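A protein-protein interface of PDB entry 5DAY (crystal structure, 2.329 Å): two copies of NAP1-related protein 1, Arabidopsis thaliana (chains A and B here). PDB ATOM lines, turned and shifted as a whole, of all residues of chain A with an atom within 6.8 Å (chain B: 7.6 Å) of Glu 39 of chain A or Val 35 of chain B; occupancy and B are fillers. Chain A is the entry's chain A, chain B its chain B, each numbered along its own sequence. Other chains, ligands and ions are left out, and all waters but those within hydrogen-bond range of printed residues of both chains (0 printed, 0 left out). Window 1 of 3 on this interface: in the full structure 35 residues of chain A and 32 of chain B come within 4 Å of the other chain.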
ATOM      1  N   GLU A  34      15.352  12.495  -5.483  1.00  0.00           N
ATOM      2  CA  GLU A  34      15.704  12.882  -4.124  1.00  0.00           C
ATOM      3  C   GLU A  34      15.026  14.180  -3.722  1.00  0.00           C
ATOM      4  O   GLU A  34      14.593  14.334  -2.571  1.00  0.00           O
ATOM      5  CB  GLU A  34      17.209  13.006  -3.990  1.00  0.00           C
ATOM      6  CG  GLU A  34      17.888  11.690  -4.122  1.00  0.00           C
ATOM      7  CD  GLU A  34      18.861  11.471  -3.012  1.00  0.00           C
ATOM      8  OE1 GLU A  34      18.442  11.633  -1.844  1.00  0.00           O
ATOM      9  OE2 GLU A  34      20.042  11.167  -3.308  1.00  0.00           O
ATOM     10  N   VAL A  35      14.941  15.120  -4.658  1.00  0.00           N
ATOM     11  CA  VAL A  35      14.176  16.338  -4.438  1.00  0.00           C
ATOM     12  C   VAL A  35      12.706  15.999  -4.206  1.00  0.00           C
ATOM     13  O   VAL A  35      12.040  16.593  -3.354  1.00  0.00           O
ATOM     14  CB  VAL A  35      14.366  17.291  -5.635  1.00  0.00           C
ATOM     15  CG1 VAL A  35      13.412  18.471  -5.548  1.00  0.00           C
ATOM     16  CG2 VAL A  35      15.820  17.754  -5.722  1.00  0.00           C
ATOM     17  N   LEU A  36      12.189  15.027  -4.952  1.00  0.00           N
ATOM     18  CA  LEU A  36      10.797  14.625  -4.818  1.00  0.00           C
ATOM     19  C   LEU A  36      10.529  13.998  -3.451  1.00  0.00           C
ATOM     20  O   LEU A  36       9.491  14.258  -2.833  1.00  0.00           O
ATOM     21  CB  LEU A  36      10.445  13.658  -5.943  1.00  0.00           C
ATOM     22  CG  LEU A  36       9.022  13.692  -6.490  1.00  0.00           C
ATOM     23  CD1 LEU A  36       8.692  15.045  -7.139  1.00  0.00           C
ATOM     24  CD2 LEU A  36       8.839  12.546  -7.472  1.00  0.00           C
ATOM     25  N   GLU A  37      11.464  13.185  -2.957  1.00  0.00           N
ATOM     26  CA  GLU A  37      11.278  12.570  -1.655  1.00  0.00           C
ATOM     27  C   GLU A  37      11.247  13.607  -0.535  1.00  0.00           C
ATOM     28  O   GLU A  37      10.515  13.427   0.442  1.00  0.00           O
ATOM     29  CB  GLU A  37      12.365  11.523  -1.425  1.00  0.00           C
ATOM     30  CG  GLU A  37      12.179  10.298  -2.326  1.00  0.00           C
ATOM     31  CD  GLU A  37      13.088   9.133  -1.975  1.00  0.00           C
ATOM     32  OE1 GLU A  37      13.970   9.301  -1.105  1.00  0.00           O
ATOM     33  OE2 GLU A  37      12.919   8.043  -2.571  1.00  0.00           O
ATOM     34  N   VAL A  38      12.024  14.691  -0.667  1.00  0.00           N
ATOM     35  CA  VAL A  38      11.971  15.793   0.289  1.00  0.00           C
ATOM     36  C   VAL A  38      10.585  16.418   0.293  1.00  0.00           C
ATOM     37  O   VAL A  38      10.041  16.735   1.356  1.00  0.00           O
ATOM     38  CB  VAL A  38      13.065  16.843  -0.021  1.00  0.00           C
ATOM     39  CG1 VAL A  38      12.899  18.086   0.855  1.00  0.00           C
ATOM     40  CG2 VAL A  38      14.470  16.251   0.163  1.00  0.00           C
ATOM     41  N   GLU A  39       9.985  16.604  -0.881  1.00  0.00           N
ATOM     42  CA  GLU A  39       8.654  17.200  -0.902  1.00  0.00           C
ATOM     43  C   GLU A  39       7.594  16.234  -0.363  1.00  0.00           C
ATOM     44  O   GLU A  39       6.665  16.654   0.338  1.00  0.00           O
ATOM     45  CB  GLU A  39       8.302  17.675  -2.309  1.00  0.00           C
ATOM     46  CG  GLU A  39       9.158  18.822  -2.812  1.00  0.00           C
ATOM     47  CD  GLU A  39       9.232  20.020  -1.851  1.00  0.00           C
ATOM     48  OE1 GLU A  39       8.281  20.257  -1.063  1.00  0.00           O
ATOM     49  OE2 GLU A  39      10.254  20.742  -1.900  1.00  0.00           O
ATOM     50  N   GLN A  40       7.726  14.941  -0.673  1.00  0.00           N
ATOM     51  CA  GLN A  40       6.821  13.939  -0.109  1.00  0.00           C
ATOM     52  C   GLN A  40       6.897  13.923   1.411  1.00  0.00           C
ATOM     53  O   GLN A  40       5.863  13.886   2.090  1.00  0.00           O
ATOM     54  CB  GLN A  40       7.154  12.563  -0.667  1.00  0.00           C
ATOM     55  CG  GLN A  40       6.816  12.401  -2.110  1.00  0.00           C
ATOM     56  CD  GLN A  40       7.582  11.267  -2.737  1.00  0.00           C
ATOM     57  OE1 GLN A  40       8.323  10.554  -2.059  1.00  0.00           O
ATOM     58  NE2 GLN A  40       7.438  11.108  -4.046  1.00  0.00           N
ATOM     59  N   LYS A  41       8.118  13.956   1.953  1.00  0.00           N
ATOM     60  CA  LYS A  41       8.300  14.002   3.393  1.00  0.00           C
ATOM     61  C   LYS A  41       7.614  15.219   4.003  1.00  0.00           C
ATOM     62  O   LYS A  41       6.994  15.111   5.059  1.00  0.00           O
ATOM     63  CB  LYS A  41       9.790  14.006   3.738  1.00  0.00           C
ATOM     64  CG  LYS A  41      10.120  14.628   5.086  1.00  0.00           C
ATOM     65  CD  LYS A  41      11.607  14.926   5.271  1.00  0.00           C
ATOM     66  CE  LYS A  41      11.864  15.569   6.620  1.00  0.00           C
ATOM     67  NZ  LYS A  41      13.298  15.563   7.030  1.00  0.00           N
ATOM     68  N   TYR A  42       7.727  16.390   3.367  1.00  0.00           N
ATOM     69  CA  TYR A  42       7.163  17.581   3.976  1.00  0.00           C
ATOM     70  C   TYR A  42       5.658  17.701   3.760  1.00  0.00           C
ATOM     71  O   TYR A  42       5.009  18.439   4.503  1.00  0.00           O
ATOM     72  CB  TYR A  42       7.894  18.838   3.488  1.00  0.00           C
ATOM     73  CG  TYR A  42       9.159  19.045   4.270  1.00  0.00           C
ATOM     74  CD1 TYR A  42       9.139  19.671   5.516  1.00  0.00           C
ATOM     75  CD2 TYR A  42      10.386  18.566   3.783  1.00  0.00           C
ATOM     76  CE1 TYR A  42      10.321  19.821   6.257  1.00  0.00           C
ATOM     77  CE2 TYR A  42      11.538  18.711   4.497  1.00  0.00           C
ATOM     78  CZ  TYR A  42      11.507  19.332   5.738  1.00  0.00           C
ATOM     79  OH  TYR A  42      12.701  19.472   6.430  1.00  0.00           O
ATOM     80  N   ASN A  43       5.085  16.993   2.781  1.00  0.00           N
ATOM     81  CA  ASN A  43       3.633  16.866   2.755  1.00  0.00           C
ATOM     82  C   ASN A  43       3.135  16.048   3.935  1.00  0.00           C
ATOM     83  O   ASN A  43       2.062  16.337   4.474  1.00  0.00           O
ATOM     84  CB  ASN A  43       3.158  16.243   1.445  1.00  0.00           C
ATOM     85  CG  ASN A  43       3.223  17.214   0.286  1.00  0.00           C
ATOM     86  OD1 ASN A  43       3.416  18.414   0.476  1.00  0.00           O
ATOM     87  ND2 ASN A  43       3.059  16.699  -0.927  1.00  0.00           N
ATOM     88  N   VAL A  44       3.900  15.043   4.356  1.00  0.00           N
ATOM     89  CA  VAL A  44       3.586  14.322   5.586  1.00  0.00           C
ATOM     90  C   VAL A  44       3.607  15.273   6.776  1.00  0.00           C
ATOM     91  O   VAL A  44       2.676  15.306   7.586  1.00  0.00           O
ATOM     92  CB  VAL A  44       4.565  13.157   5.784  1.00  0.00           C
ATOM     93  CG1 VAL A  44       4.396  12.534   7.189  1.00  0.00           C
ATOM     94  CG2 VAL A  44       4.345  12.124   4.689  1.00  0.00           C
ATOM     95  N   ARG A  46       3.322  18.568   6.913  1.00  0.00           N
ATOM     96  CA  ARG A  46       2.343  19.639   6.918  1.00  0.00           C
ATOM     97  C   ARG A  46       0.913  19.146   7.134  1.00  0.00           C
ATOM     98  O   ARG A  46       0.054  19.942   7.528  1.00  0.00           O
ATOM     99  CB  ARG A  46       2.423  20.419   5.613  1.00  0.00           C
ATOM    100  CG  ARG A  46       3.527  21.486   5.621  1.00  0.00           C
ATOM    101  CD  ARG A  46       3.559  22.287   4.334  1.00  0.00           C
ATOM    102  NE  ARG A  46       3.824  21.430   3.189  1.00  0.00           N
ATOM    103  CZ  ARG A  46       4.905  21.483   2.403  1.00  0.00           C
ATOM    104  NH1 ARG A  46       5.857  22.374   2.594  1.00  0.00           N
ATOM    105  NH2 ARG A  46       5.013  20.630   1.403  1.00  0.00           N
ATOM    106  N   ASP A  96      -1.640  17.076  -2.706  1.00  0.00           N
ATOM    107  CA  ASP A  96      -0.816  16.402  -3.700  1.00  0.00           C
ATOM    108  C   ASP A  96      -1.088  14.900  -3.697  1.00  0.00           C
ATOM    109  O   ASP A  96      -1.422  14.306  -2.668  1.00  0.00           O
ATOM    110  CB  ASP A  96       0.677  16.608  -3.414  1.00  0.00           C
ATOM    111  CG  ASP A  96       1.134  18.047  -3.575  1.00  0.00           C
ATOM    112  OD1 ASP A  96       0.666  18.752  -4.493  1.00  0.00           O
ATOM    113  OD2 ASP A  96       1.996  18.477  -2.777  1.00  0.00           O
ATOM    114  N   LYS A  98       0.262  11.186  -3.408  1.00  0.00           N
ATOM    115  CA  LYS A  98       1.247  10.663  -2.470  1.00  0.00           C
ATOM    116  C   LYS A  98       2.670  10.867  -2.981  1.00  0.00           C
ATOM    117  O   LYS A  98       3.561  11.256  -2.218  1.00  0.00           O
ATOM    118  CB  LYS A  98       0.981   9.179  -2.212  1.00  0.00           C
ATOM    119  CG  LYS A  98       1.941   8.522  -1.233  1.00  0.00           C
ATOM    120  CD  LYS A  98       1.469   8.674   0.225  1.00  0.00           C
ATOM    121  CE  LYS A  98       2.388   7.904   1.197  1.00  0.00           C
ATOM    122  NZ  LYS A  98       1.807   6.583   1.646  1.00  0.00           N
ATOM    123  N   VAL A 100       3.566  13.112  -5.255  1.00  0.00           N
ATOM    124  CA  VAL A 100       3.723  14.506  -5.668  1.00  0.00           C
ATOM    125  C   VAL A 100       3.677  14.643  -7.186  1.00  0.00           C
ATOM    126  O   VAL A 100       2.767  15.282  -7.729  1.00  0.00           O
ATOM    127  CB  VAL A 100       5.018  15.136  -5.116  1.00  0.00           C
ATOM    128  CG1 VAL A 100       5.133  16.600  -5.552  1.00  0.00           C
ATOM    129  CG2 VAL A 100       5.064  15.034  -3.615  1.00  0.00           C
ATOM    130  N   ASN B  28       8.062  25.300   5.534  1.00  0.00           N
ATOM    131  CA  ASN B  28       8.441  25.507   4.144  1.00  0.00           C
ATOM    132  C   ASN B  28       9.920  25.854   4.012  1.00  0.00           C
ATOM    133  O   ASN B  28      10.579  25.439   3.049  1.00  0.00           O
ATOM    134  CB  ASN B  28       7.575  26.599   3.530  1.00  0.00           C
ATOM    135  CG  ASN B  28       6.174  26.140   3.318  1.00  0.00           C
ATOM    136  OD1 ASN B  28       5.932  24.946   3.124  1.00  0.00           O
ATOM    137  ND2 ASN B  28       5.224  27.065   3.377  1.00  0.00           N
ATOM    138  N   GLU B  29      10.463  26.584   4.992  1.00  0.00           N
ATOM    139  CA  GLU B  29      11.865  26.965   4.958  1.00  0.00           C
ATOM    140  C   GLU B  29      12.776  25.783   5.261  1.00  0.00           C
ATOM    141  O   GLU B  29      13.872  25.681   4.692  1.00  0.00           O
ATOM    142  CB  GLU B  29      12.105  28.119   5.918  1.00  0.00           C
ATOM    143  CG  GLU B  29      11.437  29.383   5.402  1.00  0.00           C
ATOM    144  CD  GLU B  29      11.314  30.481   6.452  1.00  0.00           C
ATOM    145  OE1 GLU B  29      11.448  30.180   7.672  1.00  0.00           O
ATOM    146  OE2 GLU B  29      11.073  31.652   6.053  1.00  0.00           O
ATOM    147  N   LYS B  30      12.347  24.866   6.132  1.00  0.00           N
ATOM    148  CA  LYS B  30      13.136  23.650   6.286  1.00  0.00           C
ATOM    149  C   LYS B  30      13.089  22.801   5.031  1.00  0.00           C
ATOM    150  O   LYS B  30      14.071  22.127   4.710  1.00  0.00           O
ATOM    151  CB  LYS B  30      12.686  22.849   7.484  1.00  0.00           C
ATOM    152  CG  LYS B  30      13.105  23.495   8.771  1.00  0.00           C
ATOM    153  CD  LYS B  30      12.409  22.877   9.958  1.00  0.00           C
ATOM    154  CE  LYS B  30      12.777  23.658  11.203  1.00  0.00           C
ATOM    155  NZ  LYS B  30      12.202  23.034  12.430  1.00  0.00           N
ATOM    156  N   ALA B  31      11.999  22.879   4.271  1.00  0.00           N
ATOM    157  CA  ALA B  31      11.907  22.096   3.046  1.00  0.00           C
ATOM    158  C   ALA B  31      12.823  22.670   1.974  1.00  0.00           C
ATOM    159  O   ALA B  31      13.531  21.919   1.288  1.00  0.00           O
ATOM    160  CB  ALA B  31      10.458  22.028   2.553  1.00  0.00           C
ATOM    161  N   SER B  32      12.824  24.006   1.831  1.00  0.00           N
ATOM    162  CA  SER B  32      13.748  24.692   0.924  1.00  0.00           C
ATOM    163  C   SER B  32      15.190  24.342   1.229  1.00  0.00           C
ATOM    164  O   SER B  32      15.971  24.025   0.327  1.00  0.00           O
ATOM    165  CB  SER B  32      13.587  26.207   1.036  1.00  0.00           C
ATOM    166  OG  SER B  32      12.355  26.632   0.524  1.00  0.00           O
ATOM    167  N   ASP B  33      15.576  24.463   2.498  1.00  0.00           N
ATOM    168  CA  ASP B  33      16.937  24.137   2.881  1.00  0.00           C
ATOM    169  C   ASP B  33      17.268  22.698   2.520  1.00  0.00           C
ATOM    170  O   ASP B  33      18.367  22.415   2.038  1.00  0.00           O
ATOM    171  CB  ASP B  33      17.143  24.379   4.375  1.00  0.00           C
ATOM    172  CG  ASP B  33      17.043  25.874   4.771  1.00  0.00           C
ATOM    173  OD1 ASP B  33      17.006  26.761   3.885  1.00  0.00           O
ATOM    174  OD2 ASP B  33      17.022  26.165   5.993  1.00  0.00           O
ATOM    175  N   GLU B  34      16.318  21.776   2.704  1.00  0.00           N
ATOM    176  CA  GLU B  34      16.616  20.368   2.467  1.00  0.00           C
ATOM    177  C   GLU B  34      16.756  20.078   0.972  1.00  0.00           C
ATOM    178  O   GLU B  34      17.608  19.280   0.563  1.00  0.00           O
ATOM    179  CB  GLU B  34      15.535  19.494   3.116  1.00  0.00           C
ATOM    180  CG  GLU B  34      16.106  18.256   3.753  1.00  0.00           C
ATOM    181  CD  GLU B  34      15.162  17.522   4.681  1.00  0.00           C
ATOM    182  OE1 GLU B  34      14.897  16.339   4.398  1.00  0.00           O
ATOM    183  OE2 GLU B  34      14.697  18.078   5.700  1.00  0.00           O
ATOM    184  N   VAL B  35      15.932  20.729   0.149  1.00  0.00           N
ATOM    185  CA  VAL B  35      16.050  20.633  -1.299  1.00  0.00           C
ATOM    186  C   VAL B  35      17.352  21.276  -1.768  1.00  0.00           C
ATOM    187  O   VAL B  35      18.072  20.720  -2.612  1.00  0.00           O
ATOM    188  CB  VAL B  35      14.830  21.282  -1.974  1.00  0.00           C
ATOM    189  CG1 VAL B  35      15.068  21.477  -3.461  1.00  0.00           C
ATOM    190  CG2 VAL B  35      13.596  20.443  -1.759  1.00  0.00           C
ATOM    191  N   LEU B  36      17.672  22.462  -1.232  1.00  0.00           N
ATOM    192  CA  LEU B  36      18.941  23.103  -1.567  1.00  0.00           C
ATOM    193  C   LEU B  36      20.103  22.158  -1.298  1.00  0.00           C
ATOM    194  O   LEU B  36      20.998  22.023  -2.130  1.00  0.00           O
ATOM    195  CB  LEU B  36      19.120  24.415  -0.787  1.00  0.00           C
ATOM    196  CG  LEU B  36      20.471  25.134  -0.991  1.00  0.00           C
ATOM    197  CD1 LEU B  36      20.686  25.501  -2.456  1.00  0.00           C
ATOM    198  CD2 LEU B  36      20.639  26.371  -0.097  1.00  0.00           C
ATOM    199  N   GLU B  37      20.075  21.451  -0.168  1.00  0.00           N
ATOM    200  CA  GLU B  37      21.159  20.532   0.149  1.00  0.00           C
ATOM    201  C   GLU B  37      21.286  19.421  -0.895  1.00  0.00           C
ATOM    202  O   GLU B  37      22.405  19.005  -1.235  1.00  0.00           O
ATOM    203  CB  GLU B  37      20.952  19.946   1.540  1.00  0.00           C
ATOM    204  CG  GLU B  37      22.185  19.246   2.088  1.00  0.00           C
ATOM    205  CD  GLU B  37      21.981  18.712   3.503  1.00  0.00           C
ATOM    206  OE1 GLU B  37      20.959  19.071   4.142  1.00  0.00           O
ATOM    207  OE2 GLU B  37      22.853  17.938   3.973  1.00  0.00           O
ATOM    208  N   VAL B  38      20.153  18.924  -1.409  1.00  0.00           N
ATOM    209  CA  VAL B  38      20.181  17.907  -2.459  1.00  0.00           C
ATOM    210  C   VAL B  38      20.774  18.475  -3.749  1.00  0.00           C
ATOM    211  O   VAL B  38      21.548  17.795  -4.435  1.00  0.00           O
ATOM    212  CB  VAL B  38      18.773  17.326  -2.706  1.00  0.00           C
ATOM    213  CG1 VAL B  38      18.754  16.507  -3.998  1.00  0.00           C
ATOM    214  CG2 VAL B  38      18.286  16.466  -1.525  1.00  0.00           C
ATOM    215  N   GLU B  39      20.406  19.710  -4.117  1.00  0.00           N
ATOM    216  CA  GLU B  39      20.978  20.324  -5.316  1.00  0.00           C
ATOM    217  C   GLU B  39      22.484  20.503  -5.171  1.00  0.00           C
ATOM    218  O   GLU B  39      23.237  20.325  -6.137  1.00  0.00           O
ATOM    219  CB  GLU B  39      20.343  21.684  -5.606  1.00  0.00           C
ATOM    220  CG  GLU B  39      18.867  21.816  -5.390  1.00  0.00           C
ATOM    221  CD  GLU B  39      18.054  21.435  -6.605  1.00  0.00           C
ATOM    222  OE1 GLU B  39      18.563  20.655  -7.444  1.00  0.00           O
ATOM    223  OE2 GLU B  39      16.897  21.913  -6.715  1.00  0.00           O
ATOM    224  N   GLN B  40      22.941  20.890  -3.980  1.00  0.00           N
ATOM    225  CA  GLN B  40      24.370  21.071  -3.779  1.00  0.00           C
ATOM    226  C   GLN B  40      25.117  19.751  -3.891  1.00  0.00           C
ATOM    227  O   GLN B  40      26.193  19.688  -4.500  1.00  0.00           O
ATOM    228  CB  GLN B  40      24.629  21.725  -2.432  1.00  0.00           C
ATOM    229  CG  GLN B  40      24.319  23.184  -2.462  1.00  0.00           C
ATOM    230  CD  GLN B  40      24.223  23.773  -1.081  1.00  0.00           C
ATOM    231  OE1 GLN B  40      24.321  23.063  -0.079  1.00  0.00           O
ATOM    232  NE2 GLN B  40      24.030  25.083  -1.018  1.00  0.00           N
ATOM    233  N   LYS B  41      24.557  18.690  -3.312  1.00  0.00           N
ATOM    234  CA  LYS B  41      25.189  17.377  -3.359  1.00  0.00           C
ATOM    235  C   LYS B  41      25.399  16.923  -4.796  1.00  0.00           C
ATOM    236  O   LYS B  41      26.462  16.399  -5.144  1.00  0.00           O
ATOM    237  CB  LYS B  41      24.324  16.373  -2.592  1.00  0.00           C
ATOM    238  CG  LYS B  41      24.725  14.911  -2.743  1.00  0.00           C
ATOM    239  CD  LYS B  41      23.636  13.975  -2.214  1.00  0.00           C
ATOM    240  CE  LYS B  41      23.968  12.519  -2.503  1.00  0.00           C
ATOM    241  NZ  LYS B  41      22.990  11.572  -1.892  1.00  0.00           N
ATOM    242  N   VAL B 100      24.089  26.402  -4.735  1.00  0.00           N
ATOM    243  CA  VAL B 100      23.225  26.518  -5.901  1.00  0.00           C
ATOM    244  C   VAL B 100      22.445  27.823  -5.860  1.00  0.00           C
ATOM    245  O   VAL B 100      22.327  28.527  -6.873  1.00  0.00           O
ATOM    246  CB  VAL B 100      22.299  25.292  -5.978  1.00  0.00           C
ATOM    247  CG1 VAL B 100      21.217  25.492  -7.030  1.00  0.00           C
ATOM    248  CG2 VAL B 100      23.126  24.066  -6.273  1.00  0.00           C
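Among the printed residues, pairs that only touch across the chains: Glu 34 of chain A with Val 38 of chain B (3.8 Å), Val 35 of chain A with Val 38 of chain B (3.6 Å), Val 38 of chain A with Ala 31 of chain B (3.9 Å), Val 38 of chain A with Glu 34 of chain B (3.7 Å), Val 38 of chain A with Val 35 of chain B (3.6 Å), Glu 39 of chain A with Val 35 of chain B (3.4 Å) and Tyr 42 of chain A with Ala 31 of chain B (3.7 Å).
Printed residues of chain A that touch a printed residue of chain B: Glu 34, Val 35, Val 38, Glu 39, Lys 41, Tyr 42 and Arg 46. Printed residues of chain B that touch a printed residue of chain A: Asn 28, Lys 30, Ala 31, Glu 34, Val 35, Val 38 and Lys 41. Hydrophobic or aromatic side chains of chain B within 4 Å of the printed part of chain A: Ala 31, Val 35 and Val 38. Among the printed residues, 12 pairs touch across the chains. Among the printed residues, Asp or Glu carboxylates within 4 Å of a Lys or Arg side-chain nitrogen of the other chain: Glu 34 of chain A with Lys 41 of chain B (3.3 Å) and Lys 41 of chain A with Glu 34 of chain B (3.2 Å).
Glu 34 of chain A touches Val 38 of chain B, and with the chains exchanged Val 38 of chain A touches Glu 34 of chain B. Glu 34 of chain A touches Lys 41 of chain B, and with the chains exchanged Lys 41 of chain A touches Glu 34 of chain B. Val 35 of chain A touches Val 38 of chain B, and with the chains exchanged Val 38 of chain A touches Val 35 of chain B. Glu 39 of chain A touches Val 35 of chain B, but with the chains exchanged Val 35 of chain A does not touch Glu 39 of chain B (4.3 Å). Of the 12 pairs that touch across the chains among the printed residues, 6 have their exchanged pair printed and touching as well.
The backbone carbonyl oxygen (O) of Tyr 42 of chain A sits close to the guanidinium group (NE) of Arg 46 of chain A. The guanidinium group of Arg 46 of chain A lies within hydrogen-bond range of the side-chain amide oxygen of Asn 43 of chain A, at 2.9 Å. O of Asn 28 of chain B sits at hydrogen-bond distance from OG of Ser 32 of chain B (3.3 Å).
Of the printed residues of chain B, Glu 39 of chain A touches Val 35 (3.4 Å). Of the printed residues of chain A, Val 35 of chain B touches Val 38 (3.6 Å) and Glu 39 (3.4 Å). Printed residues of chain B within 4 Å of Arg 46 of chain A: Asn 28 (2.6 Å). Printed residues of chain B within 4 Å of Val 35 of chain A: Val 38. Of the printed residues of chain A, Asn 28 of chain B touches Arg 46 (2.6 Å). Printed residues of chain B within 4 Å of Glu 34 of chain A: Val 38 (3.8 Å) and Lys 41 (3.3 Å). Val 100 of chain B touches none of the printed residues of chain A. Leu 36 of chain B touches none of the printed residues of chain A. The nearest residue of chain B that does not touch Glu 39 of chain A is Ala 31 of chain B (4.6 Å). The nearest printed residue of chain A that does not touch Val 35 of chain B is Val 35 of chain A (4.02 Å). The nearest printed residue of chain A that does not touch Lys 41 of chain B is Val 35 of chain A (9.1 Å).
The side-chain amino group (NZ) of Lys 41 of chain B is in salt-bridge range of the side-chain carboxylate (OE2) of Glu 34 of chain A, 3.3 Å away. NZ of Lys 41 of chain A is in salt-bridge range of OE2 of Glu 34 of chain B (3.2 Å). The backbone carbonyl oxygen of Lys 30 of chain B is in hydrogen-bond range of the side-chain hydroxyl of Tyr 42 of chain A (3.4 Å). OH of Tyr 42 of chain A is in hydrogen-bond range of OE2 of Glu 34 of chain B. OD1 of Asn 28 of chain B sits at hydrogen-bond distance from NH1 of Arg 46 of chain A (2.6 Å).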
